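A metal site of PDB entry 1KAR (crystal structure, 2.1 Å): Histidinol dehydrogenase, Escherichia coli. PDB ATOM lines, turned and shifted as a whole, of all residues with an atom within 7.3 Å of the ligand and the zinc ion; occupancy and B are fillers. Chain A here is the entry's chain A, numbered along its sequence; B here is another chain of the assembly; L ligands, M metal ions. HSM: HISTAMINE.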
ATOM      1  N   LEU A 138     -19.074  10.609 -20.880  1.00  0.00           N
ATOM      2  CA  LEU A 138     -18.406  11.402 -21.904  1.00  0.00           C
ATOM      3  C   LEU A 138     -19.262  11.371 -23.173  1.00  0.00           C
ATOM      4  O   LEU A 138     -18.881  10.745 -24.169  1.00  0.00           O
ATOM      5  CB  LEU A 138     -17.004  10.854 -22.178  1.00  0.00           C
ATOM      6  CG  LEU A 138     -15.880  11.339 -21.245  1.00  0.00           C
ATOM      7  CD1 LEU A 138     -16.262  11.111 -19.798  1.00  0.00           C
ATOM      8  CD2 LEU A 138     -14.588  10.618 -21.586  1.00  0.00           C
ATOM      9  N   PHE A 139     -20.397  12.045 -23.121  1.00  0.00           N
ATOM     10  CA  PHE A 139     -21.331  12.083 -24.261  1.00  0.00           C
ATOM     11  C   PHE A 139     -20.721  12.660 -25.536  1.00  0.00           C
ATOM     12  O   PHE A 139     -21.248  12.437 -26.619  1.00  0.00           O
ATOM     13  CB  PHE A 139     -22.587  12.884 -23.891  1.00  0.00           C
ATOM     14  CG  PHE A 139     -22.329  14.333 -23.633  1.00  0.00           C
ATOM     15  CD1 PHE A 139     -22.196  15.231 -24.694  1.00  0.00           C
ATOM     16  CD2 PHE A 139     -22.177  14.812 -22.339  1.00  0.00           C
ATOM     17  CE1 PHE A 139     -21.927  16.577 -24.471  1.00  0.00           C
ATOM     18  CE2 PHE A 139     -21.904  16.149 -22.093  1.00  0.00           C
ATOM     19  CZ  PHE A 139     -21.774  17.034 -23.173  1.00  0.00           C
ATOM     20  N   SER A 140     -19.612  13.384 -25.414  1.00  0.00           N
ATOM     21  CA  SER A 140     -18.962  13.961 -26.580  1.00  0.00           C
ATOM     22  C   SER A 140     -18.547  12.871 -27.569  1.00  0.00           C
ATOM     23  O   SER A 140     -18.542  13.086 -28.779  1.00  0.00           O
ATOM     24  CB  SER A 140     -17.733  14.798 -26.167  1.00  0.00           C
ATOM     25  OG  SER A 140     -16.800  14.042 -25.404  1.00  0.00           O
ATOM     26  N   THR A 141     -18.201  11.697 -27.049  1.00  0.00           N
ATOM     27  CA  THR A 141     -17.804  10.583 -27.906  1.00  0.00           C
ATOM     28  C   THR A 141     -18.966  10.194 -28.850  1.00  0.00           C
ATOM     29  O   THR A 141     -18.745   9.619 -29.922  1.00  0.00           O
ATOM     30  CB  THR A 141     -17.406   9.365 -27.065  1.00  0.00           C
ATOM     31  OG1 THR A 141     -16.431   9.761 -26.093  1.00  0.00           O
ATOM     32  CG2 THR A 141     -16.807   8.287 -27.938  1.00  0.00           C
ATOM     33  N   MET A 144     -18.588  12.170 -31.873  1.00  0.00           N
ATOM     34  CA  MET A 144     -17.402  11.693 -32.594  1.00  0.00           C
ATOM     35  C   MET A 144     -17.604  10.398 -33.393  1.00  0.00           C
ATOM     36  O   MET A 144     -16.952  10.183 -34.411  1.00  0.00           O
ATOM     37  CB  MET A 144     -16.240  11.475 -31.623  1.00  0.00           C
ATOM     38  CG  MET A 144     -15.735  12.730 -30.942  1.00  0.00           C
ATOM     39  SD  MET A 144     -15.143  14.071 -32.203  1.00  0.00           S
ATOM     40  CE  MET A 144     -15.021  15.580 -30.978  1.00  0.00           C
ATOM     41  N   PRO A 209     -14.577   2.940 -27.125  1.00  0.00           N
ATOM     42  CA  PRO A 209     -13.805   2.322 -26.053  1.00  0.00           C
ATOM     43  C   PRO A 209     -14.628   2.127 -24.790  1.00  0.00           C
ATOM     44  O   PRO A 209     -15.736   2.654 -24.678  1.00  0.00           O
ATOM     45  CB  PRO A 209     -12.664   3.314 -25.850  1.00  0.00           C
ATOM     46  CG  PRO A 209     -13.367   4.638 -26.080  1.00  0.00           C
ATOM     47  CD  PRO A 209     -14.164   4.346 -27.319  1.00  0.00           C
ATOM     48  N   SER A 237      -4.506   6.163 -22.619  1.00  0.00           N
ATOM     49  CA  SER A 237      -4.402   7.416 -23.360  1.00  0.00           C
ATOM     50  C   SER A 237      -3.050   8.073 -23.116  1.00  0.00           C
ATOM     51  O   SER A 237      -2.448   7.858 -22.071  1.00  0.00           O
ATOM     52  CB  SER A 237      -5.511   8.382 -22.944  1.00  0.00           C
ATOM     53  OG  SER A 237      -6.780   7.818 -23.216  1.00  0.00           O
ATOM     54  N   SER A 258      -5.097  17.895 -18.149  1.00  0.00           N
ATOM     55  CA  SER A 258      -6.287  17.532 -18.911  1.00  0.00           C
ATOM     56  C   SER A 258      -6.187  16.045 -19.226  1.00  0.00           C
ATOM     57  O   SER A 258      -7.134  15.287 -19.046  1.00  0.00           O
ATOM     58  CB  SER A 258      -6.352  18.304 -20.243  1.00  0.00           C
ATOM     59  OG  SER A 258      -6.714  19.656 -20.055  1.00  0.00           O
ATOM     60  N   GLN A 259      -5.014  15.645 -19.694  1.00  0.00           N
ATOM     61  CA  GLN A 259      -4.781  14.250 -20.030  1.00  0.00           C
ATOM     62  C   GLN A 259      -4.821  13.367 -18.798  1.00  0.00           C
ATOM     63  O   GLN A 259      -5.452  12.320 -18.799  1.00  0.00           O
ATOM     64  CB  GLN A 259      -3.435  14.085 -20.725  1.00  0.00           C
ATOM     65  CG  GLN A 259      -3.177  12.669 -21.169  1.00  0.00           C
ATOM     66  CD  GLN A 259      -4.248  12.155 -22.098  1.00  0.00           C
ATOM     67  OE1 GLN A 259      -4.950  11.194 -21.794  1.00  0.00           O
ATOM     68  NE2 GLN A 259      -4.387  12.796 -23.248  1.00  0.00           N
ATOM     69  N   GLU A 261      -6.344  13.701 -15.918  1.00  0.00           N
ATOM     70  CA  GLU A 261      -7.650  13.492 -15.298  1.00  0.00           C
ATOM     71  C   GLU A 261      -8.542  12.484 -16.033  1.00  0.00           C
ATOM     72  O   GLU A 261      -9.661  12.219 -15.591  1.00  0.00           O
ATOM     73  CB  GLU A 261      -8.404  14.821 -15.125  1.00  0.00           C
ATOM     74  CG  GLU A 261      -8.928  15.481 -16.400  1.00  0.00           C
ATOM     75  CD  GLU A 261      -9.881  16.656 -16.115  1.00  0.00           C
ATOM     76  OE1 GLU A 261      -9.989  17.064 -14.946  1.00  0.00           O
ATOM     77  OE2 GLU A 261     -10.513  17.165 -17.058  1.00  0.00           O
ATOM     78  N   HIS A 262      -8.053  11.911 -17.123  1.00  0.00           N
ATOM     79  CA  HIS A 262      -8.832  10.919 -17.853  1.00  0.00           C
ATOM     80  C   HIS A 262      -8.785   9.554 -17.152  1.00  0.00           C
ATOM     81  O   HIS A 262      -9.767   8.814 -17.173  1.00  0.00           O
ATOM     82  CB  HIS A 262      -8.332  10.766 -19.285  1.00  0.00           C
ATOM     83  CG  HIS A 262      -9.048  11.627 -20.274  1.00  0.00           C
ATOM     84  ND1 HIS A 262     -10.418  11.655 -20.375  1.00  0.00           N
ATOM     85  CD2 HIS A 262      -8.589  12.510 -21.197  1.00  0.00           C
ATOM     86  CE1 HIS A 262     -10.779  12.502 -21.320  1.00  0.00           C
ATOM     87  NE2 HIS A 262      -9.686  13.044 -21.833  1.00  0.00           N
ATOM     88  N   GLU A 326      -0.290   9.531 -28.779  1.00  0.00           N
ATOM     89  CA  GLU A 326      -1.675   9.668 -29.173  1.00  0.00           C
ATOM     90  C   GLU A 326      -1.959  11.143 -29.480  1.00  0.00           C
ATOM     91  O   GLU A 326      -2.470  11.475 -30.556  1.00  0.00           O
ATOM     92  CB  GLU A 326      -2.588   9.211 -28.044  1.00  0.00           C
ATOM     93  CG  GLU A 326      -4.060   9.282 -28.406  1.00  0.00           C
ATOM     94  CD  GLU A 326      -4.967   9.125 -27.192  1.00  0.00           C
ATOM     95  OE1 GLU A 326      -4.453   8.940 -26.071  1.00  0.00           O
ATOM     96  OE2 GLU A 326      -6.202   9.193 -27.366  1.00  0.00           O
ATOM     97  N   HIS A 327      -1.636  12.021 -28.530  1.00  0.00           N
ATOM     98  CA  HIS A 327      -1.799  13.462 -28.709  1.00  0.00           C
ATOM     99  C   HIS A 327      -0.415  14.084 -28.626  1.00  0.00           C
ATOM    100  O   HIS A 327       0.314  13.824 -27.669  1.00  0.00           O
ATOM    101  CB  HIS A 327      -2.647  14.107 -27.602  1.00  0.00           C
ATOM    102  CG  HIS A 327      -3.984  13.472 -27.391  1.00  0.00           C
ATOM    103  ND1 HIS A 327      -4.188  12.433 -26.499  1.00  0.00           N
ATOM    104  CD2 HIS A 327      -5.208  13.786 -27.889  1.00  0.00           C
ATOM    105  CE1 HIS A 327      -5.477  12.146 -26.452  1.00  0.00           C
ATOM    106  NE2 HIS A 327      -6.110  12.951 -27.283  1.00  0.00           N
ATOM    107  N   GLU A 356      -5.652  20.666 -25.689  1.00  0.00           N
ATOM    108  CA  GLU A 356      -6.142  19.334 -25.983  1.00  0.00           C
ATOM    109  C   GLU A 356      -7.676  19.369 -25.967  1.00  0.00           C
ATOM    110  O   GLU A 356      -8.330  18.830 -26.874  1.00  0.00           O
ATOM    111  CB  GLU A 356      -5.630  18.331 -24.935  1.00  0.00           C
ATOM    112  CG  GLU A 356      -6.207  16.921 -25.094  1.00  0.00           C
ATOM    113  CD  GLU A 356      -5.581  15.930 -24.144  1.00  0.00           C
ATOM    114  OE1 GLU A 356      -5.646  16.150 -22.916  1.00  0.00           O
ATOM    115  OE2 GLU A 356      -5.018  14.917 -24.616  1.00  0.00           O
ATOM    116  N   SER A 357      -8.235  20.005 -24.940  1.00  0.00           N
ATOM    117  CA  SER A 357      -9.686  20.106 -24.770  1.00  0.00           C
ATOM    118  C   SER A 357     -10.401  20.690 -25.979  1.00  0.00           C
ATOM    119  O   SER A 357     -11.586  20.431 -26.180  1.00  0.00           O
ATOM    120  CB  SER A 357     -10.011  20.933 -23.511  1.00  0.00           C
ATOM    121  OG  SER A 357      -9.314  22.169 -23.514  1.00  0.00           O
ATOM    122  N   GLY A 359      -9.567  20.041 -29.117  1.00  0.00           N
ATOM    123  CA  GLY A 359      -9.730  18.922 -30.027  1.00  0.00           C
ATOM    124  C   GLY A 359     -10.715  17.898 -29.503  1.00  0.00           C
ATOM    125  O   GLY A 359     -11.406  17.232 -30.284  1.00  0.00           O
ATOM    126  N   ASP A 360     -10.777  17.728 -28.192  1.00  0.00           N
ATOM    127  CA  ASP A 360     -11.726  16.774 -27.602  1.00  0.00           C
ATOM    128  C   ASP A 360     -13.175  17.183 -27.877  1.00  0.00           C
ATOM    129  O   ASP A 360     -14.044  16.325 -28.053  1.00  0.00           O
ATOM    130  CB  ASP A 360     -11.558  16.675 -26.071  1.00  0.00           C
ATOM    131  CG  ASP A 360     -10.255  16.007 -25.648  1.00  0.00           C
ATOM    132  OD1 ASP A 360      -9.717  15.173 -26.405  1.00  0.00           O
ATOM    133  OD2 ASP A 360      -9.779  16.312 -24.531  1.00  0.00           O
ATOM    134  N   TYR A 361     -13.433  18.495 -27.910  1.00  0.00           N
ATOM    135  CA  TYR A 361     -14.811  18.972 -28.064  1.00  0.00           C
ATOM    136  C   TYR A 361     -15.303  19.752 -29.275  1.00  0.00           C
ATOM    137  O   TYR A 361     -16.394  19.474 -29.772  1.00  0.00           O
ATOM    138  CB  TYR A 361     -15.189  19.796 -26.836  1.00  0.00           C
ATOM    139  CG  TYR A 361     -15.094  19.087 -25.516  1.00  0.00           C
ATOM    140  CD1 TYR A 361     -14.108  19.418 -24.595  1.00  0.00           C
ATOM    141  CD2 TYR A 361     -16.014  18.092 -25.177  1.00  0.00           C
ATOM    142  CE1 TYR A 361     -14.027  18.774 -23.358  1.00  0.00           C
ATOM    143  CE2 TYR A 361     -15.943  17.439 -23.937  1.00  0.00           C
ATOM    144  CZ  TYR A 361     -14.941  17.790 -23.039  1.00  0.00           C
ATOM    145  OH  TYR A 361     -14.864  17.154 -21.824  1.00  0.00           O
ATOM    146  N   HIS A 367     -11.715  12.866 -31.609  1.00  0.00           N
ATOM    147  CA  HIS A 367     -10.943  12.562 -30.401  1.00  0.00           C
ATOM    148  C   HIS A 367     -10.796  11.061 -30.153  1.00  0.00           C
ATOM    149  O   HIS A 367     -10.288  10.654 -29.112  1.00  0.00           O
ATOM    150  CB  HIS A 367     -11.538  13.279 -29.186  1.00  0.00           C
ATOM    151  CG  HIS A 367     -12.809  12.675 -28.653  1.00  0.00           C
ATOM    152  ND1 HIS A 367     -13.747  13.427 -27.973  1.00  0.00           N
ATOM    153  CD2 HIS A 367     -13.266  11.398 -28.631  1.00  0.00           C
ATOM    154  CE1 HIS A 367     -14.723  12.638 -27.553  1.00  0.00           C
ATOM    155  NE2 HIS A 367     -14.455  11.405 -27.951  1.00  0.00           N
ATOM    156  N   VAL A 368     -11.252  10.251 -31.102  1.00  0.00           N
ATOM    157  CA  VAL A 368     -11.119   8.800 -30.993  1.00  0.00           C
ATOM    158  C   VAL A 368      -9.847   8.500 -31.781  1.00  0.00           C
ATOM    159  O   VAL A 368      -9.862   8.463 -33.013  1.00  0.00           O
ATOM    160  CB  VAL A 368     -12.308   8.051 -31.634  1.00  0.00           C
ATOM    161  CG1 VAL A 368     -12.047   6.540 -31.615  1.00  0.00           C
ATOM    162  CG2 VAL A 368     -13.585   8.390 -30.878  1.00  0.00           C
ATOM    163  N   LEU A 369      -8.767   8.276 -31.051  1.00  0.00           N
ATOM    164  CA  LEU A 369      -7.462   8.084 -31.673  1.00  0.00           C
ATOM    165  C   LEU A 369      -6.688   6.828 -31.322  1.00  0.00           C
ATOM    166  O   LEU A 369      -6.921   6.194 -30.295  1.00  0.00           O
ATOM    167  CB  LEU A 369      -6.580   9.289 -31.312  1.00  0.00           C
ATOM    168  CG  LEU A 369      -7.230  10.668 -31.391  1.00  0.00           C
ATOM    169  CD1 LEU A 369      -6.438  11.655 -30.533  1.00  0.00           C
ATOM    170  CD2 LEU A 369      -7.291  11.108 -32.832  1.00  0.00           C
ATOM    171  N   LEU B 410     -19.080  22.261 -22.631  1.00  0.00           N
ATOM    172  CA  LEU B 410     -19.010  20.814 -22.830  1.00  0.00           C
ATOM    173  C   LEU B 410     -18.132  20.132 -21.774  1.00  0.00           C
ATOM    174  O   LEU B 410     -18.515  19.100 -21.224  1.00  0.00           O
ATOM    175  CB  LEU B 410     -18.490  20.519 -24.249  1.00  0.00           C
ATOM    176  CG  LEU B 410     -19.397  21.109 -25.349  1.00  0.00           C
ATOM    177  CD1 LEU B 410     -18.786  20.884 -26.708  1.00  0.00           C
ATOM    178  CD2 LEU B 410     -20.768  20.462 -25.262  1.00  0.00           C
ATOM    179  N   ALA B 411     -16.988  20.736 -21.488  1.00  0.00           N
ATOM    180  CA  ALA B 411     -16.063  20.189 -20.495  1.00  0.00           C
ATOM    181  C   ALA B 411     -16.750  20.124 -19.135  1.00  0.00           C
ATOM    182  O   ALA B 411     -16.663  19.103 -18.438  1.00  0.00           O
ATOM    183  CB  ALA B 411     -14.832  21.071 -20.409  1.00  0.00           C
ATOM    184  N   GLU B 414     -19.168  17.324 -18.840  1.00  0.00           N
ATOM    185  CA  GLU B 414     -18.578  15.997 -18.652  1.00  0.00           C
ATOM    186  C   GLU B 414     -17.826  15.936 -17.323  1.00  0.00           C
ATOM    187  O   GLU B 414     -17.153  14.946 -17.037  1.00  0.00           O
ATOM    188  CB  GLU B 414     -17.620  15.645 -19.801  1.00  0.00           C
ATOM    189  CG  GLU B 414     -18.236  15.703 -21.195  1.00  0.00           C
ATOM    190  CD  GLU B 414     -17.418  14.969 -22.242  1.00  0.00           C
ATOM    191  OE1 GLU B 414     -16.178  15.093 -22.246  1.00  0.00           O
ATOM    192  OE2 GLU B 414     -18.024  14.263 -23.079  1.00  0.00           O
ATOM    193  N   LEU B 416     -15.145  17.422 -16.340  1.00  0.00           N
ATOM    194  CA  LEU B 416     -13.706  17.323 -16.542  1.00  0.00           C
ATOM    195  C   LEU B 416     -13.171  18.726 -16.314  1.00  0.00           C
ATOM    196  O   LEU B 416     -12.934  19.495 -17.260  1.00  0.00           O
ATOM    197  CB  LEU B 416     -13.395  16.857 -17.974  1.00  0.00           C
ATOM    198  CG  LEU B 416     -13.786  15.403 -18.279  1.00  0.00           C
ATOM    199  CD1 LEU B 416     -13.338  15.053 -19.683  1.00  0.00           C
ATOM    200  CD2 LEU B 416     -13.123  14.467 -17.265  1.00  0.00           C
ATOM    201  N   HIS B 419      -9.998  20.060 -17.995  1.00  0.00           N
ATOM    202  CA  HIS B 419     -10.230  20.330 -19.407  1.00  0.00           C
ATOM    203  C   HIS B 419     -10.784  21.745 -19.505  1.00  0.00           C
ATOM    204  O   HIS B 419     -10.427  22.503 -20.395  1.00  0.00           O
ATOM    205  CB  HIS B 419     -11.251  19.362 -20.010  1.00  0.00           C
ATOM    206  CG  HIS B 419     -10.658  18.056 -20.451  1.00  0.00           C
ATOM    207  ND1 HIS B 419     -10.207  17.106 -19.561  1.00  0.00           N
ATOM    208  CD2 HIS B 419     -10.485  17.536 -21.693  1.00  0.00           C
ATOM    209  CE1 HIS B 419      -9.786  16.046 -20.239  1.00  0.00           C
ATOM    210  NE2 HIS B 419      -9.947  16.284 -21.531  1.00  0.00           N
HETATM  211  N   HSM L   1      -9.772  10.369 -25.042  1.00  0.00           N
HETATM  212  CA  HSM L   1     -11.129  10.926 -24.984  1.00  0.00           C
HETATM  213  CB  HSM L   1     -11.134  12.442 -25.255  1.00  0.00           C
HETATM  214  CG  HSM L   1     -12.137  13.205 -24.435  1.00  0.00           C
HETATM  215  ND1 HSM L   1     -11.751  14.268 -23.647  1.00  0.00           N
HETATM  216  CD2 HSM L   1     -13.487  13.093 -24.283  1.00  0.00           C
HETATM  217  CE1 HSM L   1     -12.841  14.864 -23.170  1.00  0.00           C
HETATM  218  NE2 HSM L   1     -13.906  14.140 -23.503  1.00  0.00           N
HETATM  219 ZN    ZN M   1      -9.853  14.831 -23.064  1.00  0.00          ZN
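NE2 of the ligand sits at hydrogen-bond distance from OE1 of Glu 414 of chain B, 2.8 Å away.
A nitrogen (NE2) of the ligand lies within hydrogen-bond range of the side-chain hydroxyl (OG) of Ser 140, 3.5 Å away.
O of Asp 360 sits at hydrogen-bond distance from ND1 of His 367, 2.9 Å away.
A ring nitrogen (ND1) of His 419 of chain B sits at hydrogen-bond distance from the side-chain carboxylate of Glu 261 (2.5 Å).
The side-chain carboxylate (OE2) of Glu 414 of chain B sits at hydrogen-bond distance from the side-chain hydroxyl (OG) of Ser 140 (2.6 Å).
The backbone NH of Phe 139 is in hydrogen-bond range of the side-chain carboxylate of Glu 414 of chain B, at 3.2 Å.
NE2 of His 367 sits at hydrogen-bond distance from OG1 of Thr 141 (3.2 Å).
N of His 367 sits at hydrogen-bond distance from SD of Met 144 (3.7 Å).
The backbone NH of Leu 416 of chain B sits at hydrogen-bond distance from the backbone carbonyl oxygen of Ala 411 of chain B, 3.1 Å away.
O of Leu 138 is in hydrogen-bond range of OG1 of Thr 141.
Merely in contact with the ligand: Leu 138 (3.8 Å), Tyr 361 (3.3 Å), His 367 (3.5 Å) and Leu 416 of chain B (3.5 Å).
Hydrophobic or aromatic side chains that line the ligand: Leu 138, His 262, Tyr 361, His 367, Leu 416 of chain B and His 419 of chain B.
Of the 26 residues printed, 9 come within 4 Å of the ligand.
The nearest printed residue that does not touch the ligand is Ser 237 (4.3 Å).
Along chain A the residues within 4 Å of the zinc ion span positions 262 to 360.
The nearest printed residue that does not touch the zinc ion is Glu 356 (4.4 Å).
The zinc ion is bound by a nitrogen (ND1) of the ligand, at 2.1 Å.
The zinc ion is bound by OD2 of Asp 360, at 2.1 Å.
NE2 of His 419 of chain B is bound to the zinc ion, at 2.1 Å.
The zinc ion is bound by NE2 of His 262, 2.2 Å away.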
